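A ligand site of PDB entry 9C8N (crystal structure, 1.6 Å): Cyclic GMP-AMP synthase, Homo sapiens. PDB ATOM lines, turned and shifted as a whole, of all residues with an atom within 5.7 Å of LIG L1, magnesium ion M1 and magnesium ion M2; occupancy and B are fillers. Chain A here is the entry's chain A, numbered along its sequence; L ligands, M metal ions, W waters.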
ATOM      1  N   GLY A  57       4.084  21.447  14.109  1.00  0.00           N
ATOM      2  CA  GLY A  57       4.226  22.216  15.342  1.00  0.00           C
ATOM      3  C   GLY A  57       3.182  21.881  16.405  1.00  0.00           C
ATOM      4  O   GLY A  57       2.352  20.974  16.286  1.00  0.00           O
ATOM      5  N   SER A  58       3.263  22.642  17.507  1.00  0.00           N
ATOM      6  CA  SER A  58       2.624  22.166  18.737  1.00  0.00           C
ATOM      7  C   SER A  58       1.101  22.130  18.648  1.00  0.00           C
ATOM      8  O   SER A  58       0.506  21.286  19.309  1.00  0.00           O
ATOM      9  CB  SER A  58       3.047  23.013  19.918  1.00  0.00           C
ATOM     10  OG  SER A  58       2.569  24.362  19.819  1.00  0.00           O
ATOM     11  N   TYR A  59       0.466  23.049  17.883  1.00  0.00           N
ATOM     12  CA  TYR A  59      -0.992  22.994  17.817  1.00  0.00           C
ATOM     13  C   TYR A  59      -1.437  21.661  17.213  1.00  0.00           C
ATOM     14  O   TYR A  59      -2.295  20.970  17.773  1.00  0.00           O
ATOM     15  CB  TYR A  59      -1.533  24.155  16.956  1.00  0.00           C
ATOM     16  CG  TYR A  59      -3.053  24.146  16.900  1.00  0.00           C
ATOM     17  CD1 TYR A  59      -3.818  24.768  17.849  1.00  0.00           C
ATOM     18  CD2 TYR A  59      -3.691  23.510  15.847  1.00  0.00           C
ATOM     19  CE1 TYR A  59      -5.171  24.747  17.805  1.00  0.00           C
ATOM     20  CE2 TYR A  59      -5.102  23.431  15.792  1.00  0.00           C
ATOM     21  CZ  TYR A  59      -5.793  24.085  16.806  1.00  0.00           C
ATOM     22  OH  TYR A  59      -7.184  24.086  16.772  1.00  0.00           O
ATOM     23  N   LYS A  64       0.246  22.380  22.234  1.00  0.00           N
ATOM     24  CA  LYS A  64       0.217  23.832  22.446  1.00  0.00           C
ATOM     25  C   LYS A  64      -0.360  24.101  23.838  1.00  0.00           C
ATOM     26  O   LYS A  64      -1.357  23.481  24.203  1.00  0.00           O
ATOM     27  CB  LYS A  64      -0.668  24.466  21.351  1.00  0.00           C
ATOM     28  CG  LYS A  64      -0.777  26.024  21.437  1.00  0.00           C
ATOM     29  CD  LYS A  64       0.423  26.696  20.849  1.00  0.00           C
ATOM     30  CE  LYS A  64       0.420  28.211  21.044  1.00  0.00           C
ATOM     31  NZ  LYS A  64       0.606  28.590  22.502  1.00  0.00           N
ATOM     32  N   GLU A  70      -0.596  30.453  18.308  1.00  0.00           N
ATOM     33  CA  GLU A  70       0.574  30.330  17.428  1.00  0.00           C
ATOM     34  C   GLU A  70       0.509  29.008  16.697  1.00  0.00           C
ATOM     35  O   GLU A  70       0.481  27.917  17.312  1.00  0.00           O
ATOM     36  CB  GLU A  70       1.883  30.420  18.230  1.00  0.00           C
ATOM     37  CG  GLU A  70       3.096  30.838  17.370  1.00  0.00           C
ATOM     38  CD  GLU A  70       3.933  29.677  16.854  1.00  0.00           C
ATOM     39  OE1 GLU A  70       3.628  28.517  17.188  1.00  0.00           O
ATOM     40  OE2 GLU A  70       4.945  29.951  16.114  1.00  0.00           O
ATOM     41  N   PHE A  71       0.491  29.112  15.373  1.00  0.00           N
ATOM     42  CA  PHE A  71       0.300  27.973  14.474  1.00  0.00           C
ATOM     43  C   PHE A  71       1.474  27.915  13.512  1.00  0.00           C
ATOM     44  O   PHE A  71       1.950  28.955  13.069  1.00  0.00           O
ATOM     45  CB  PHE A  71      -1.002  28.133  13.636  1.00  0.00           C
ATOM     46  CG  PHE A  71      -2.262  28.041  14.407  1.00  0.00           C
ATOM     47  CD1 PHE A  71      -2.659  29.076  15.280  1.00  0.00           C
ATOM     48  CD2 PHE A  71      -3.095  26.944  14.196  1.00  0.00           C
ATOM     49  CE1 PHE A  71      -3.855  28.972  16.000  1.00  0.00           C
ATOM     50  CE2 PHE A  71      -4.294  26.819  14.929  1.00  0.00           C
ATOM     51  CZ  PHE A  71      -4.660  27.857  15.813  1.00  0.00           C
ATOM     52  N   ASP A  72       1.871  26.706  13.119  1.00  0.00           N
ATOM     53  CA  ASP A  72       2.994  26.489  12.212  1.00  0.00           C
ATOM     54  C   ASP A  72       2.559  25.662  11.028  1.00  0.00           C
ATOM     55  O   ASP A  72       1.970  24.587  11.211  1.00  0.00           O
ATOM     56  CB  ASP A  72       4.111  25.773  12.972  1.00  0.00           C
ATOM     57  CG  ASP A  72       4.545  26.540  14.206  1.00  0.00           C
ATOM     58  OD1 ASP A  72       5.198  27.595  14.046  1.00  0.00           O
ATOM     59  OD2 ASP A  72       4.146  26.092  15.321  1.00  0.00           O
ATOM     60  N   TYR A  93      22.742  21.235   6.676  1.00  0.00           N
ATOM     61  CA  TYR A  93      22.567  22.245   5.631  1.00  0.00           C
ATOM     62  C   TYR A  93      23.125  21.751   4.319  1.00  0.00           C
ATOM     63  O   TYR A  93      24.166  21.066   4.291  1.00  0.00           O
ATOM     64  CB  TYR A  93      23.238  23.575   5.999  1.00  0.00           C
ATOM     65  CG  TYR A  93      22.710  24.198   7.267  1.00  0.00           C
ATOM     66  CD1 TYR A  93      21.615  25.057   7.196  1.00  0.00           C
ATOM     67  CD2 TYR A  93      23.262  23.917   8.511  1.00  0.00           C
ATOM     68  CE1 TYR A  93      21.098  25.657   8.356  1.00  0.00           C
ATOM     69  CE2 TYR A  93      22.752  24.544   9.682  1.00  0.00           C
ATOM     70  CZ  TYR A  93      21.680  25.403   9.556  1.00  0.00           C
ATOM     71  OH  TYR A  93      21.133  25.989  10.678  1.00  0.00           O
ATOM     72  N   SER A 150      15.132  32.777  10.754  1.00  0.00           N
ATOM     73  CA  SER A 150      13.959  31.901  10.636  1.00  0.00           C
ATOM     74  C   SER A 150      13.697  31.577   9.172  1.00  0.00           C
ATOM     75  O   SER A 150      13.860  32.441   8.294  1.00  0.00           O
ATOM     76  CB  SER A 150      12.729  32.574  11.219  1.00  0.00           C
ATOM     77  OG  SER A 150      11.563  31.781  10.952  1.00  0.00           O
ATOM     78  N   PRO A 151      13.260  30.349   8.861  1.00  0.00           N
ATOM     79  CA  PRO A 151      12.881  30.079   7.477  1.00  0.00           C
ATOM     80  C   PRO A 151      11.457  30.514   7.161  1.00  0.00           C
ATOM     81  O   PRO A 151      11.025  30.351   6.030  1.00  0.00           O
ATOM     82  CB  PRO A 151      13.010  28.555   7.372  1.00  0.00           C
ATOM     83  CG  PRO A 151      12.578  28.073   8.745  1.00  0.00           C
ATOM     84  CD  PRO A 151      13.206  29.120   9.690  1.00  0.00           C
ATOM     85  N   ALA A 152      10.703  30.998   8.149  1.00  0.00           N
ATOM     86  CA  ALA A 152       9.286  31.285   7.977  1.00  0.00           C
ATOM     87  C   ALA A 152       8.994  32.737   7.546  1.00  0.00           C
ATOM     88  O   ALA A 152       9.791  33.668   7.763  1.00  0.00           O
ATOM     89  CB  ALA A 152       8.562  30.972   9.289  1.00  0.00           C
ATOM     90  N   ASP A 164       3.313  30.964  11.454  1.00  0.00           N
ATOM     91  CA  ASP A 164       4.585  30.783  10.742  1.00  0.00           C
ATOM     92  C   ASP A 164       4.326  29.956   9.499  1.00  0.00           C
ATOM     93  O   ASP A 164       3.818  28.829   9.602  1.00  0.00           O
ATOM     94  CB  ASP A 164       5.619  30.037  11.590  1.00  0.00           C
ATOM     95  CG  ASP A 164       6.146  30.891  12.706  1.00  0.00           C
ATOM     96  OD1 ASP A 164       6.405  32.107  12.495  1.00  0.00           O
ATOM     97  OD2 ASP A 164       6.336  30.371  13.816  1.00  0.00           O
ATOM     98  N   THR A 166       6.228  28.300   6.460  1.00  0.00           N
ATOM     99  CA  THR A 166       7.567  27.942   6.018  1.00  0.00           C
ATOM    100  C   THR A 166       7.497  27.278   4.654  1.00  0.00           C
ATOM    101  O   THR A 166       6.922  26.206   4.479  1.00  0.00           O
ATOM    102  CB  THR A 166       8.262  27.050   7.043  1.00  0.00           C
ATOM    103  OG1 THR A 166       8.393  27.788   8.242  1.00  0.00           O
ATOM    104  CG2 THR A 166       9.645  26.645   6.569  1.00  0.00           C
ATOM    105  N   VAL A 205      14.119  23.575   4.039  1.00  0.00           N
ATOM    106  CA  VAL A 205      13.479  24.862   4.330  1.00  0.00           C
ATOM    107  C   VAL A 205      14.567  25.923   4.192  1.00  0.00           C
ATOM    108  O   VAL A 205      15.744  25.609   4.360  1.00  0.00           O
ATOM    109  CB  VAL A 205      12.801  24.873   5.724  1.00  0.00           C
ATOM    110  CG1 VAL A 205      11.729  23.779   5.816  1.00  0.00           C
ATOM    111  CG2 VAL A 205      13.833  24.719   6.899  1.00  0.00           C
ATOM    112  N   LYS A 207      16.456  28.088   5.701  1.00  0.00           N
ATOM    113  CA  LYS A 207      17.233  28.552   6.830  1.00  0.00           C
ATOM    114  C   LYS A 207      18.685  28.302   6.452  1.00  0.00           C
ATOM    115  O   LYS A 207      19.053  27.161   6.121  1.00  0.00           O
ATOM    116  CB  LYS A 207      16.884  27.808   8.112  1.00  0.00           C
ATOM    117  CG  LYS A 207      17.844  28.279   9.237  1.00  0.00           C
ATOM    118  CD  LYS A 207      17.493  27.683  10.527  1.00  0.00           C
ATOM    119  CE  LYS A 207      18.535  28.027  11.597  1.00  0.00           C
ATOM    120  NZ  LYS A 207      18.616  29.502  11.718  1.00  0.00           N
ATOM    121  N   ARG A 221      17.994  23.902   4.798  1.00  0.00           N
ATOM    122  CA  ARG A 221      18.112  23.149   6.040  1.00  0.00           C
ATOM    123  C   ARG A 221      17.136  21.983   6.033  1.00  0.00           C
ATOM    124  O   ARG A 221      15.981  22.142   5.614  1.00  0.00           O
ATOM    125  CB  ARG A 221      17.835  24.125   7.167  1.00  0.00           C
ATOM    126  CG  ARG A 221      17.565  23.515   8.492  1.00  0.00           C
ATOM    127  CD  ARG A 221      18.802  23.001   9.084  1.00  0.00           C
ATOM    128  NE  ARG A 221      18.513  22.291  10.324  1.00  0.00           N
ATOM    129  CZ  ARG A 221      18.722  22.733  11.558  1.00  0.00           C
ATOM    130  NH1 ARG A 221      19.227  23.945  11.805  1.00  0.00           N
ATOM    131  NH2 ARG A 221      18.440  21.945  12.580  1.00  0.00           N
ATOM    132  N   LEU A 222      17.617  20.808   6.434  1.00  0.00           N
ATOM    133  CA  LEU A 222      16.759  19.625   6.524  1.00  0.00           C
ATOM    134  C   LEU A 222      15.696  19.817   7.604  1.00  0.00           C
ATOM    135  O   LEU A 222      16.000  20.301   8.712  1.00  0.00           O
ATOM    136  CB  LEU A 222      17.566  18.410   6.920  1.00  0.00           C
ATOM    137  CG  LEU A 222      18.420  17.747   5.876  1.00  0.00           C
ATOM    138  CD1 LEU A 222      19.150  16.539   6.516  1.00  0.00           C
ATOM    139  CD2 LEU A 222      17.526  17.293   4.668  1.00  0.00           C
ATOM    140  N   SER A 223      14.472  19.415   7.287  1.00  0.00           N
ATOM    141  CA  SER A 223      13.396  19.481   8.260  1.00  0.00           C
ATOM    142  C   SER A 223      12.602  18.178   8.255  1.00  0.00           C
ATOM    143  O   SER A 223      12.215  17.660   7.189  1.00  0.00           O
ATOM    144  CB  SER A 223      12.462  20.656   7.970  1.00  0.00           C
ATOM    145  OG  SER A 223      11.347  20.656   8.862  1.00  0.00           O
ATOM    146  N   PHE A 224      12.314  17.684   9.467  1.00  0.00           N
ATOM    147  CA  PHE A 224      11.492  16.488   9.638  1.00  0.00           C
ATOM    148  C   PHE A 224      10.312  16.799  10.565  1.00  0.00           C
ATOM    149  O   PHE A 224       9.840  15.929  11.320  1.00  0.00           O
ATOM    150  CB  PHE A 224      12.298  15.288  10.170  1.00  0.00           C
ATOM    151  CG  PHE A 224      13.466  14.903   9.277  1.00  0.00           C
ATOM    152  CD1 PHE A 224      13.279  14.007   8.209  1.00  0.00           C
ATOM    153  CD2 PHE A 224      14.729  15.493   9.456  1.00  0.00           C
ATOM    154  CE1 PHE A 224      14.298  13.689   7.349  1.00  0.00           C
ATOM    155  CE2 PHE A 224      15.753  15.167   8.592  1.00  0.00           C
ATOM    156  CZ  PHE A 224      15.524  14.228   7.561  1.00  0.00           C
ATOM    157  N   SER A 225       9.790  18.030  10.493  1.00  0.00           N
ATOM    158  CA  SER A 225       8.662  18.426  11.335  1.00  0.00           C
ATOM    159  C   SER A 225       7.484  17.494  11.162  1.00  0.00           C
ATOM    160  O   SER A 225       6.729  17.245  12.112  1.00  0.00           O
ATOM    161  CB  SER A 225       8.196  19.857  11.010  1.00  0.00           C
ATOM    162  OG  SER A 225       9.213  20.777  11.259  1.00  0.00           O
HETATM  163  C1  LIG L   1      13.673  24.103  10.759  1.00  0.00           C
HETATM  164  C2  LIG L   1      11.529  25.178  11.072  1.00  0.00           C
HETATM  165  C3  LIG L   1      11.655  27.282  12.599  1.00  0.00           C
HETATM  166  C4  LIG L   1       7.627  30.828  17.326  1.00  0.00           C
HETATM  167  C5  LIG L   1       9.050  30.075  15.629  1.00  0.00           C
HETATM  168  C6  LIG L   1       9.114  28.957  14.568  1.00  0.00           C
HETATM  169  C7  LIG L   1      11.374  29.729  13.989  1.00  0.00           C
HETATM  170  C8  LIG L   1      12.701  28.997  14.172  1.00  0.00           C
HETATM  171  C9  LIG L   1      12.739  27.802  13.275  1.00  0.00           C
HETATM  172  C10 LIG L   1      13.543  26.052  12.087  1.00  0.00           C
HETATM  173  C11 LIG L   1      14.256  25.044  11.531  1.00  0.00           C
HETATM  174  C12 LIG L   1      12.235  24.141  10.515  1.00  0.00           C
HETATM  175  C13 LIG L   1      12.111  26.128  11.880  1.00  0.00           C
HETATM  176  C14 LIG L   1      10.260  27.795  12.782  1.00  0.00           C
HETATM  177  C15 LIG L   1       9.663  28.311  11.400  1.00  0.00           C
HETATM  178  N1  LIG L   1      10.211  28.787  13.833  1.00  0.00           N
HETATM  179  N2  LIG L   1      13.909  27.081  12.945  1.00  0.00           N
HETATM  180  O1  LIG L   1       7.782  29.987  16.206  1.00  0.00           O
HETATM  181  O2  LIG L   1       8.106  28.259  14.347  1.00  0.00           O
HETATM  182 CL1  LIG L   1      14.543  22.757  10.077  1.00  0.00          CL
HETATM  183 CL2  LIG L   1      15.962  25.013  11.867  1.00  0.00          CL
HETATM  184  P1  LG2 L   2       5.373  26.287  20.536  1.00  0.00           P
HETATM  185  O1  LG2 L   2       4.232  25.705  21.324  1.00  0.00           O
HETATM  186  O2  LG2 L   2       6.424  27.032  21.319  1.00  0.00           O
HETATM  187  O3  LG2 L   2       4.913  27.038  19.315  1.00  0.00           O
HETATM  188  P2  LG2 L   2       6.364  24.351  18.548  1.00  0.00           P
HETATM  189  O4  LG2 L   2       6.946  23.012  18.290  1.00  0.00           O
HETATM  190  O5  LG2 L   2       5.389  24.812  17.512  1.00  0.00           O
HETATM  191  N1  LG2 L   2       6.157  24.824  20.079  1.00  0.00           N
HETATM  192  P3  LG2 L   2       7.803  26.594  17.117  1.00  0.00           P
HETATM  193  O6  LG2 L   2       8.962  27.472  17.355  1.00  0.00           O
HETATM  194  O7  LG2 L   2       6.559  27.207  16.578  1.00  0.00           O
HETATM  195  O8  LG2 L   2       7.735  25.375  18.048  1.00  0.00           O
HETATM  196  O9  LG2 L   2       8.382  25.730  15.637  1.00  0.00           O
HETATM  197  C1  LG2 L   2       7.488  25.020  14.951  1.00  0.00           C
HETATM  198  C2  LG2 L   2       8.137  23.745  14.415  1.00  0.00           C
HETATM  199  O10 LG2 L   2       9.263  24.121  13.638  1.00  0.00           O
HETATM  200  C3  LG2 L   2       8.696  22.869  15.548  1.00  0.00           C
HETATM  201  O11 LG2 L   2       7.758  22.002  16.014  1.00  0.00           O
HETATM  202  C4  LG2 L   2       9.778  22.082  14.748  1.00  0.00           C
HETATM  203  O12 LG2 L   2       9.121  21.111  14.021  1.00  0.00           O
HETATM  204  C5  LG2 L   2      10.274  23.179  13.774  1.00  0.00           C
HETATM  205  N2  LG2 L   2      11.425  23.814  14.376  1.00  0.00           N
HETATM  206  C6  LG2 L   2      11.495  24.938  15.219  1.00  0.00           C
HETATM  207  N3  LG2 L   2      12.746  25.166  15.592  1.00  0.00           N
HETATM  208  C7  LG2 L   2      13.506  24.190  15.004  1.00  0.00           C
HETATM  209  C8  LG2 L   2      14.852  23.903  15.016  1.00  0.00           C
HETATM  210  N4  LG2 L   2      15.716  24.697  15.727  1.00  0.00           N
HETATM  211  N5  LG2 L   2      15.353  22.860  14.342  1.00  0.00           N
HETATM  212  C9  LG2 L   2      14.457  22.129  13.670  1.00  0.00           C
HETATM  213  N6  LG2 L   2      13.145  22.269  13.552  1.00  0.00           N
HETATM  214  C10 LG2 L   2      12.698  23.313  14.245  1.00  0.00           C
HETATM  215 MG    MG M   1       6.306  28.822  15.172  1.00  0.00          MG
HETATM  216 MG    MG M   2       4.487  26.657  17.277  1.00  0.00          MG
HETATM  217  O   HOH W   1       9.398  32.095  12.638  1.00  0.00           O
HETATM  218  O   HOH W   2       7.112  30.980  20.654  1.00  0.00           O
HETATM  219  O   HOH W   3      16.236  27.948  14.436  1.00  0.00           O
HETATM  220  O   HOH W   4       2.522  26.015  17.652  1.00  0.00           O
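The backbone NH of Ser 58 sits close to an oxygen (O5) of LG2 L2 (3.0 Å). An oxygen (O1) of LG2 L2 sits at hydrogen-bond distance from the side-chain hydroxyl (OG) of Ser 58. An oxygen (O12) of LG2 L2 sits at hydrogen-bond distance from the side-chain hydroxyl of Ser 225, at 2.8 Å.
The backbone carbonyl oxygen (O) of Phe 71 sits at hydrogen-bond distance from the backbone NH (N) of Asp 164, 2.9 Å away. The backbone carbonyl oxygen of Arg 221 lies within hydrogen-bond range of the backbone NH of Val 205, 2.8 Å away. NH1 of Arg 221 lies within hydrogen-bond range of OH of Tyr 93, at 3.0 Å. The backbone NH of Ala 152 is in hydrogen-bond range of the side-chain hydroxyl of Ser 150. The side-chain hydroxyl of Ser 225 is in hydrogen-bond range of the side-chain hydroxyl of Ser 223. The backbone carbonyl oxygen (O) of Ser 58 sits at hydrogen-bond distance from the backbone NH (N) of Lys 64, 3.1 Å away.
OG of Ser 150 touches C7 of LIG L1, 3.7 Å away. Pro 151 touches LIG L1 (CG to C13, 3.7 Å). Ala 152 touches LIG L1 (CB to C15, 3.6 Å). OG1 of Thr 166 touches C15 of LIG L1, 3.4 Å away. CG2 of Val 205 touches CL1 of LIG L1 (3.8 Å). Lys 207 touches LIG L1 (CD to CL2, 3.4 Å). NH1 of Arg 221 touches CL2 of LIG L1 (3.4 Å). Leu 222 touches LIG L1. CB of Ser 223 touches CL1 of LIG L1, at 3.6 Å. 12 residues have an atom within 4 Å of LIG L1: Glu 70, Asp 72, Ser 150, Pro 151, Ala 152, Asp 164, Thr 166, Val 205, Lys 207, Arg 221, Leu 222 and Ser 223. The nearest printed residue that does not touch LIG L1 is Ser 225 (4.6 Å).
Of the 20 residues printed, 3 come within 4 Å of magnesium ion M1. Along chain A the residues within 4 Å of magnesium ion M1 span positions 70 to 164.
Merely in contact with magnesium ion M2: Ser 58 (3.9 Å). Within 4 Å of magnesium ion M2: Ser 58, Glu 70 and Asp 72. Along chain A the residues within 4 Å of magnesium ion M2 span positions 58 to 72.
Magnesium ion M1 is bound by OD1 of Asp 72 (2.0 Å), OE2 of Glu 70 (2.0 Å), OD2 of Asp 164 (2.1 Å), O2 of LIG L1 (2.1 Å), O1 of LIG L1 (2.1 Å) and O7 of LG2 L2 (2.2 Å). Magnesium ion M1 has six donor atoms within binding distance.
OE1 of Glu 70 is bound to magnesium ion M2 (2.1 Å). OD2 of Asp 72 binds magnesium ion M2 (2.1 Å). Magnesium ion M2 is bound by O5 of LG2 L2 (2.1 Å). Water W4 binds magnesium ion M2 (2.1 Å). An oxygen (O3) of LG2 L2 is bound to magnesium ion M2 (2.1 Å). Magnesium ion M2 is bound by O7 of LG2 L2 (2.3 Å). Magnesium ion M2 has six donor atoms within binding distance.
Water W4 lies within hydrogen-bond range of the side-chain hydroxyl (OG) of Ser 58 (2.7 Å) and the backbone carbonyl oxygen (O) of Glu 70 (2.8 Å). Water W1 bridges OG of Ser 150 and OD1 of Asp 164.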
